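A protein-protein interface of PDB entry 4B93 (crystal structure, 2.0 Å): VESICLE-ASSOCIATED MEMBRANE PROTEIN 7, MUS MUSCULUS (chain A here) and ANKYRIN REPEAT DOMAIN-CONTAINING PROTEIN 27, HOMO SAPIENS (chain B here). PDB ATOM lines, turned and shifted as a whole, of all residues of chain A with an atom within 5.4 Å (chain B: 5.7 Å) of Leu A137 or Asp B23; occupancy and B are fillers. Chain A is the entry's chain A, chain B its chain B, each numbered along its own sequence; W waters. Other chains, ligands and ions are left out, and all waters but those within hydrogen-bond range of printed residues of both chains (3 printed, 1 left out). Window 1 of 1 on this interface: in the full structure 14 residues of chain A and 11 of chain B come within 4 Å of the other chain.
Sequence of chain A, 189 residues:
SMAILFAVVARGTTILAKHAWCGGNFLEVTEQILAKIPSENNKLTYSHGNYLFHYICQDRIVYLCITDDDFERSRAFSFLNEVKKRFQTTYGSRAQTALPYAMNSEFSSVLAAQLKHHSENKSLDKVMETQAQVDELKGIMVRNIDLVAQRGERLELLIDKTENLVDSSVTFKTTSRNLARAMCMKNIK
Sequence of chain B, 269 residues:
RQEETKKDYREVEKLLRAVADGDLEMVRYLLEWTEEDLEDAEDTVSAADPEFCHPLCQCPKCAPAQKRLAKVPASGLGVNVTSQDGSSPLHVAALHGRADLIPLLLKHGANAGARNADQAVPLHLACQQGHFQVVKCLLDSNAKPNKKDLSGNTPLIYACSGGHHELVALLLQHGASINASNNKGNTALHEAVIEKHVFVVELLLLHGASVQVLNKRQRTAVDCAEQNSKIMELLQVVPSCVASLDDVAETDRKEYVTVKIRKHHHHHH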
ATOM      1  N   ARG A  73     -31.496 -13.634  28.180  1.00  0.00           N
ATOM      2  CA  ARG A  73     -32.157 -12.940  27.071  1.00  0.00           C
ATOM      3  C   ARG A  73     -31.986 -13.601  25.733  1.00  0.00           C
ATOM      4  O   ARG A  73     -32.886 -13.555  24.889  1.00  0.00           O
ATOM      5  CB  ARG A  73     -31.721 -11.480  27.006  1.00  0.00           C
ATOM      6  CG  ARG A  73     -32.213 -10.670  28.184  1.00  0.00           C
ATOM      7  CD  ARG A  73     -32.553  -9.262  27.800  1.00  0.00           C
ATOM      8  NE  ARG A  73     -31.383  -8.555  27.327  1.00  0.00           N
ATOM      9  CZ  ARG A  73     -31.399  -7.399  26.687  1.00  0.00           C
ATOM     10  NH1 ARG A  73     -32.567  -6.798  26.382  1.00  0.00           N
ATOM     11  NH2 ARG A  73     -30.239  -6.872  26.291  1.00  0.00           N
ATOM     12  N   SER A  74     -30.837 -14.242  25.495  1.00  0.00           N
ATOM     13  CA  SER A  74     -30.636 -14.878  24.201  1.00  0.00           C
ATOM     14  C   SER A  74     -31.649 -15.923  23.934  1.00  0.00           C
ATOM     15  O   SER A  74     -32.129 -16.070  22.807  1.00  0.00           O
ATOM     16  CB  SER A  74     -29.209 -15.496  24.044  1.00  0.00           C
ATOM     17  OG  SER A  74     -28.780 -16.225  25.200  1.00  0.00           O
ATOM     18  N   PHE A  77     -35.080 -14.198  23.233  1.00  0.00           N
ATOM     19  CA  PHE A  77     -35.238 -13.616  21.913  1.00  0.00           C
ATOM     20  C   PHE A  77     -35.265 -14.621  20.815  1.00  0.00           C
ATOM     21  O   PHE A  77     -35.940 -14.444  19.790  1.00  0.00           O
ATOM     22  CB  PHE A  77     -34.318 -12.432  21.697  1.00  0.00           C
ATOM     23  CG  PHE A  77     -34.834 -11.185  22.341  1.00  0.00           C
ATOM     24  CD1 PHE A  77     -35.789 -10.443  21.738  1.00  0.00           C
ATOM     25  CD2 PHE A  77     -34.410 -10.814  23.570  1.00  0.00           C
ATOM     26  CE1 PHE A  77     -36.311  -9.312  22.347  1.00  0.00           C
ATOM     27  CE2 PHE A  77     -34.915  -9.707  24.188  1.00  0.00           C
ATOM     28  CZ  PHE A  77     -35.869  -8.939  23.580  1.00  0.00           C
ATOM     29  N   GLN A 133     -27.708 -15.888  17.957  1.00  0.00           N
ATOM     30  CA  GLN A 133     -28.561 -15.690  19.148  1.00  0.00           C
ATOM     31  C   GLN A 133     -28.070 -14.708  20.227  1.00  0.00           C
ATOM     32  O   GLN A 133     -28.884 -14.043  20.872  1.00  0.00           O
ATOM     33  CB  GLN A 133     -28.820 -17.027  19.832  1.00  0.00           C
ATOM     34  CG  GLN A 133     -29.742 -17.918  19.050  1.00  0.00           C
ATOM     35  CD  GLN A 133     -30.023 -19.214  19.781  1.00  0.00           C
ATOM     36  OE1 GLN A 133     -29.837 -19.317  21.001  1.00  0.00           O
ATOM     37  NE2 GLN A 133     -30.489 -20.211  19.040  1.00  0.00           N
ATOM     38  N   VAL A 134     -26.761 -14.641  20.451  1.00  0.00           N
ATOM     39  CA  VAL A 134     -26.211 -13.668  21.405  1.00  0.00           C
ATOM     40  C   VAL A 134     -26.007 -12.251  20.764  1.00  0.00           C
ATOM     41  O   VAL A 134     -26.067 -11.209  21.473  1.00  0.00           O
ATOM     42  CB  VAL A 134     -24.915 -14.221  22.036  1.00  0.00           C
ATOM     43  CG1 VAL A 134     -24.304 -13.203  23.004  1.00  0.00           C
ATOM     44  CG2 VAL A 134     -25.194 -15.560  22.707  1.00  0.00           C
ATOM     45  N   ASP A 135     -25.783 -12.205  19.441  1.00  0.00           N
ATOM     46  CA  ASP A 135     -25.612 -10.919  18.732  1.00  0.00           C
ATOM     47  C   ASP A 135     -26.945 -10.255  18.428  1.00  0.00           C
ATOM     48  O   ASP A 135     -27.004  -9.040  18.161  1.00  0.00           O
ATOM     49  CB  ASP A 135     -24.804 -11.135  17.472  1.00  0.00           C
ATOM     50  CG  ASP A 135     -23.424 -11.694  17.796  1.00  0.00           C
ATOM     51  OD1 ASP A 135     -22.872 -11.300  18.851  1.00  0.00           O
ATOM     52  OD2 ASP A 135     -22.908 -12.554  17.046  1.00  0.00           O
ATOM     53  N   GLU A 136     -28.010 -11.062  18.474  1.00  0.00           N
ATOM     54  CA  GLU A 136     -29.380 -10.534  18.488  1.00  0.00           C
ATOM     55  C   GLU A 136     -29.527  -9.394  19.509  1.00  0.00           C
ATOM     56  O   GLU A 136     -30.171  -8.377  19.235  1.00  0.00           O
ATOM     57  CB  GLU A 136     -30.349 -11.650  18.810  1.00  0.00           C
ATOM     58  CG  GLU A 136     -31.780 -11.211  18.973  1.00  0.00           C
ATOM     59  CD  GLU A 136     -32.442 -10.837  17.680  1.00  0.00           C
ATOM     60  OE1 GLU A 136     -32.042 -11.354  16.634  1.00  0.00           O
ATOM     61  OE2 GLU A 136     -33.394 -10.056  17.718  1.00  0.00           O
ATOM     62  N   LEU A 137     -28.853  -9.556  20.643  1.00  0.00           N
ATOM     63  CA  LEU A 137     -29.072  -8.766  21.800  1.00  0.00           C
ATOM     64  C   LEU A 137     -28.481  -7.419  21.732  1.00  0.00           C
ATOM     65  O   LEU A 137     -28.563  -6.653  22.726  1.00  0.00           O
ATOM     66  CB  LEU A 137     -28.452  -9.431  23.022  1.00  0.00           C
ATOM     67  CG  LEU A 137     -28.907 -10.843  23.314  1.00  0.00           C
ATOM     68  CD1 LEU A 137     -28.251 -11.283  24.610  1.00  0.00           C
ATOM     69  CD2 LEU A 137     -30.415 -10.912  23.443  1.00  0.00           C
ATOM     70  N   LYS A 138     -27.844  -7.127  20.613  1.00  0.00           N
ATOM     71  CA  LYS A 138     -27.065  -5.920  20.541  1.00  0.00           C
ATOM     72  C   LYS A 138     -28.005  -4.773  20.419  1.00  0.00           C
ATOM     73  O   LYS A 138     -28.896  -4.788  19.594  1.00  0.00           O
ATOM     74  CB  LYS A 138     -26.116  -5.919  19.347  1.00  0.00           C
ATOM     75  CG  LYS A 138     -24.662  -5.847  19.753  1.00  0.00           C
ATOM     76  CD  LYS A 138     -23.868  -7.077  19.309  1.00  0.00           C
ATOM     77  CE  LYS A 138     -22.565  -6.660  18.630  1.00  0.00           C
ATOM     78  NZ  LYS A 138     -21.670  -7.819  18.414  1.00  0.00           N
ATOM     79  N   GLY A 139     -27.786  -3.755  21.211  1.00  0.00           N
ATOM     80  CA  GLY A 139     -28.811  -2.682  21.302  1.00  0.00           C
ATOM     81  C   GLY A 139     -30.301  -3.035  21.646  1.00  0.00           C
ATOM     82  O   GLY A 139     -31.226  -2.364  21.208  1.00  0.00           O
ATOM     83  N   ILE A 140     -30.566  -4.119  22.360  1.00  0.00           N
ATOM     84  CA  ILE A 140     -31.910  -4.283  22.966  1.00  0.00           C
ATOM     85  C   ILE A 140     -31.766  -3.828  24.369  1.00  0.00           C
ATOM     86  O   ILE A 140     -31.166  -4.507  25.166  1.00  0.00           O
ATOM     87  CB  ILE A 140     -32.392  -5.713  22.934  1.00  0.00           C
ATOM     88  CG1 ILE A 140     -32.255  -6.278  21.530  1.00  0.00           C
ATOM     89  CG2 ILE A 140     -33.848  -5.766  23.368  1.00  0.00           C
ATOM     90  CD1 ILE A 140     -32.920  -7.633  21.350  1.00  0.00           C
ATOM     91  N   ALA B  18     -25.639 -12.661  33.003  1.00  0.00           N
ATOM     92  CA  ALA B  18     -25.768 -11.737  31.864  1.00  0.00           C
ATOM     93  C   ALA B  18     -24.376 -11.664  31.117  1.00  0.00           C
ATOM     94  O   ALA B  18     -24.302 -11.862  29.919  1.00  0.00           O
ATOM     95  CB  ALA B  18     -26.219 -10.370  32.331  1.00  0.00           C
ATOM     96  N   VAL B  19     -23.313 -11.367  31.864  1.00  0.00           N
ATOM     97  CA  VAL B  19     -21.909 -11.498  31.355  1.00  0.00           C
ATOM     98  C   VAL B  19     -21.738 -12.790  30.511  1.00  0.00           C
ATOM     99  O   VAL B  19     -21.425 -12.755  29.319  1.00  0.00           O
ATOM    100  CB  VAL B  19     -20.931 -11.512  32.530  1.00  0.00           C
ATOM    101  CG1 VAL B  19     -19.490 -11.712  32.036  1.00  0.00           C
ATOM    102  CG2 VAL B  19     -21.015 -10.204  33.307  1.00  0.00           C
ATOM    103  N   ALA B  20     -22.010 -13.920  31.127  1.00  0.00           N
ATOM    104  CA  ALA B  20     -21.869 -15.212  30.452  1.00  0.00           C
ATOM    105  C   ALA B  20     -22.635 -15.341  29.164  1.00  0.00           C
ATOM    106  O   ALA B  20     -22.149 -15.922  28.226  1.00  0.00           O
ATOM    107  CB  ALA B  20     -22.219 -16.338  31.396  1.00  0.00           C
ATOM    108  N   ASP B  21     -23.792 -14.701  29.067  1.00  0.00           N
ATOM    109  CA  ASP B  21     -24.631 -14.744  27.844  1.00  0.00           C
ATOM    110  C   ASP B  21     -24.207 -13.669  26.849  1.00  0.00           C
ATOM    111  O   ASP B  21     -24.827 -13.491  25.793  1.00  0.00           O
ATOM    112  CB  ASP B  21     -26.109 -14.503  28.296  1.00  0.00           C
ATOM    113  CG  ASP B  21     -27.134 -14.835  27.231  1.00  0.00           C
ATOM    114  OD1 ASP B  21     -27.004 -15.859  26.578  1.00  0.00           O
ATOM    115  OD2 ASP B  21     -28.093 -14.072  27.045  1.00  0.00           O
ATOM    116  N   GLY B  22     -23.170 -12.901  27.197  1.00  0.00           N
ATOM    117  CA  GLY B  22     -22.672 -11.859  26.330  1.00  0.00           C
ATOM    118  C   GLY B  22     -23.621 -10.700  26.219  1.00  0.00           C
ATOM    119  O   GLY B  22     -23.691 -10.057  25.182  1.00  0.00           O
ATOM    120  N   ASP B  23     -24.336 -10.402  27.292  1.00  0.00           N
ATOM    121  CA  ASP B  23     -25.439  -9.451  27.216  1.00  0.00           C
ATOM    122  C   ASP B  23     -25.039  -8.099  27.722  1.00  0.00           C
ATOM    123  O   ASP B  23     -25.205  -7.790  28.920  1.00  0.00           O
ATOM    124  CB  ASP B  23     -26.601  -9.935  28.067  1.00  0.00           C
ATOM    125  CG  ASP B  23     -27.958  -9.298  27.661  1.00  0.00           C
ATOM    126  OD1 ASP B  23     -27.975  -8.151  27.163  1.00  0.00           O
ATOM    127  OD2 ASP B  23     -29.010  -9.979  27.866  1.00  0.00           O
ATOM    128  N   LEU B  24     -24.574  -7.261  26.803  1.00  0.00           N
ATOM    129  CA  LEU B  24     -24.026  -5.961  27.182  1.00  0.00           C
ATOM    130  C   LEU B  24     -25.092  -5.008  27.769  1.00  0.00           C
ATOM    131  O   LEU B  24     -24.833  -4.303  28.759  1.00  0.00           O
ATOM    132  CB  LEU B  24     -23.339  -5.302  25.990  1.00  0.00           C
ATOM    133  CG  LEU B  24     -22.877  -3.845  26.220  1.00  0.00           C
ATOM    134  CD1 LEU B  24     -21.905  -3.752  27.367  1.00  0.00           C
ATOM    135  CD2 LEU B  24     -22.270  -3.222  24.964  1.00  0.00           C
ATOM    136  N   GLU B  25     -26.263  -4.925  27.142  1.00  0.00           N
ATOM    137  CA  GLU B  25     -27.287  -4.019  27.712  1.00  0.00           C
ATOM    138  C   GLU B  25     -27.793  -4.491  29.110  1.00  0.00           C
ATOM    139  O   GLU B  25     -28.002  -3.678  30.048  1.00  0.00           O
ATOM    140  CB  GLU B  25     -28.405  -3.844  26.746  1.00  0.00           C
ATOM    141  CG  GLU B  25     -28.078  -3.091  25.472  1.00  0.00           C
ATOM    142  CD  GLU B  25     -27.372  -1.802  25.725  1.00  0.00           C
ATOM    143  OE1 GLU B  25     -27.647  -1.105  26.735  1.00  0.00           O
ATOM    144  OE2 GLU B  25     -26.499  -1.501  24.901  1.00  0.00           O
ATOM    145  N   MET B  26     -27.916  -5.795  29.305  1.00  0.00           N
ATOM    146  CA  MET B  26     -28.210  -6.251  30.634  1.00  0.00           C
ATOM    147  C   MET B  26     -27.109  -5.891  31.633  1.00  0.00           C
ATOM    148  O   MET B  26     -27.395  -5.373  32.756  1.00  0.00           O
ATOM    149  CB  MET B  26     -28.574  -7.737  30.695  1.00  0.00           C
ATOM    150  CG  MET B  26     -28.937  -8.168  32.136  1.00  0.00           C
ATOM    151  SD  MET B  26     -30.487  -7.400  32.777  1.00  0.00           S
ATOM    152  CE  MET B  26     -31.557  -8.222  31.647  1.00  0.00           C
ATOM    153  N   VAL B  27     -25.848  -6.137  31.278  1.00  0.00           N
ATOM    154  CA  VAL B  27     -24.769  -5.780  32.195  1.00  0.00           C
ATOM    155  C   VAL B  27     -24.856  -4.319  32.523  1.00  0.00           C
ATOM    156  O   VAL B  27     -24.654  -3.901  33.663  1.00  0.00           O
ATOM    157  CB  VAL B  27     -23.358  -6.083  31.584  1.00  0.00           C
ATOM    158  CG1 VAL B  27     -22.240  -5.341  32.329  1.00  0.00           C
ATOM    159  CG2 VAL B  27     -23.100  -7.572  31.587  1.00  0.00           C
ATOM    160  N   ARG B  28     -25.089  -3.520  31.501  1.00  0.00           N
ATOM    161  CA  ARG B  28     -25.197  -2.068  31.689  1.00  0.00           C
ATOM    162  C   ARG B  28     -26.328  -1.666  32.650  1.00  0.00           C
ATOM    163  O   ARG B  28     -26.171  -0.754  33.470  1.00  0.00           O
ATOM    164  CB  ARG B  28     -25.453  -1.398  30.345  1.00  0.00           C
ATOM    165  CG  ARG B  28     -25.260   0.101  30.364  1.00  0.00           C
ATOM    166  CD  ARG B  28     -25.992   0.829  29.233  1.00  0.00           C
ATOM    167  NE  ARG B  28     -25.756   0.237  27.912  1.00  0.00           N
ATOM    168  CZ  ARG B  28     -24.587   0.258  27.266  1.00  0.00           C
ATOM    169  NH1 ARG B  28     -23.525   0.839  27.802  1.00  0.00           N
ATOM    170  NH2 ARG B  28     -24.476  -0.292  26.061  1.00  0.00           N
ATOM    171  N   LEU B 101     -17.551  -7.751  25.556  1.00  0.00           N
ATOM    172  CA  LEU B 101     -17.656  -7.148  26.902  1.00  0.00           C
ATOM    173  C   LEU B 101     -16.394  -6.616  27.532  1.00  0.00           C
ATOM    174  O   LEU B 101     -16.434  -5.736  28.412  1.00  0.00           O
ATOM    175  CB  LEU B 101     -18.257  -8.111  27.897  1.00  0.00           C
ATOM    176  CG  LEU B 101     -19.633  -8.634  27.633  1.00  0.00           C
ATOM    177  CD1 LEU B 101     -20.073  -9.289  28.910  1.00  0.00           C
ATOM    178  CD2 LEU B 101     -20.570  -7.515  27.240  1.00  0.00           C
HETATM  179  O   HOH W   1     -27.031  -6.424  24.961  1.00  0.00           O
HETATM  180  O   HOH W   2     -29.030 -12.188  29.012  1.00  0.00           O
HETATM  181  O   HOH W   3     -25.959  -3.243  22.762  1.00  0.00           O
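NH2 of Arg A73 lies within salt-bridge range of OD1 of Asp B23 (2.7 Å).
OG of Ser A74 lies within hydrogen-bond range of OD2 of Asp B21 (2.9 Å).
The guanidinium group (NH2) of Arg A73 is in hydrogen-bond range of the backbone carbonyl oxygen (O) of Ile A140, at 2.8 Å.
The backbone carbonyl oxygen (O) of Ala B18 is in hydrogen-bond range of the backbone NH (N) of Asp B23 (3.0 Å).
OD1 of Asp B23 lies within hydrogen-bond range of N of Met B26, 3.2 Å away.
The side-chain carboxylate of Glu B25 is in salt-bridge range of the guanidinium group of Arg B28 (2.6 Å).
Among the printed residues, pairs that only touch across the chains: Arg A73 with Asp B21, Arg A73 with Glu B25, Arg A73 with Met B26, Val A134 with Asp B21, Val A134 with Gly B22, Leu A137 with Asp B21, Leu A137 with Asp B23 and Ile A140 with Glu B25.
Leu A137 touches just these residues of chain B: Asp B21 (3.7 Å) and Asp B23 (3.6 Å).
Of chain A, only Arg A73 and Leu A137 come within 4 Å of Asp B23.
Printed residues of chain A within 4 Å of Glu B25: Arg A73 and Ile A140.
Of the printed residues of chain B, Val A134 touches Asp B21 and Gly B22.
The nearest residue of chain A that does not touch Asp B23 is Val A134 (5.1 Å).
The nearest printed residue of chain A that does not touch Asp B21 is Gln A133 (6.2 Å).
Hydrophobic or aromatic side chains of chain A within 4 Å of the printed part of chain B: Val A134 and Leu A137.
Of the 12 printed residues of chain B, 5 touch a printed residue of chain A.
Printed residues of chain B that touch a printed residue of chain A: Asp B21, Gly B22, Asp B23, Glu B25 and Met B26.
Among the printed residues, 10 pairs touch across the chains.
Water W3 bridges the backbone NH of Gly A139 and the side-chain carboxylate of Glu B25.
Water W2 lies within hydrogen-bond range of OD2 of Asp B23 (2.5 Å), OD2 of Asp B21 (2.9 Å) and N of Arg A73 (3.0 Å).
Water W1 lies within hydrogen-bond range of the backbone carbonyl oxygen of Leu A137 (2.7 Å), the backbone NH of Glu B25 (2.8 Å), the side-chain carboxylate of Asp B23 (3.0 Å) and the backbone NH of Leu B24 (3.2 Å).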
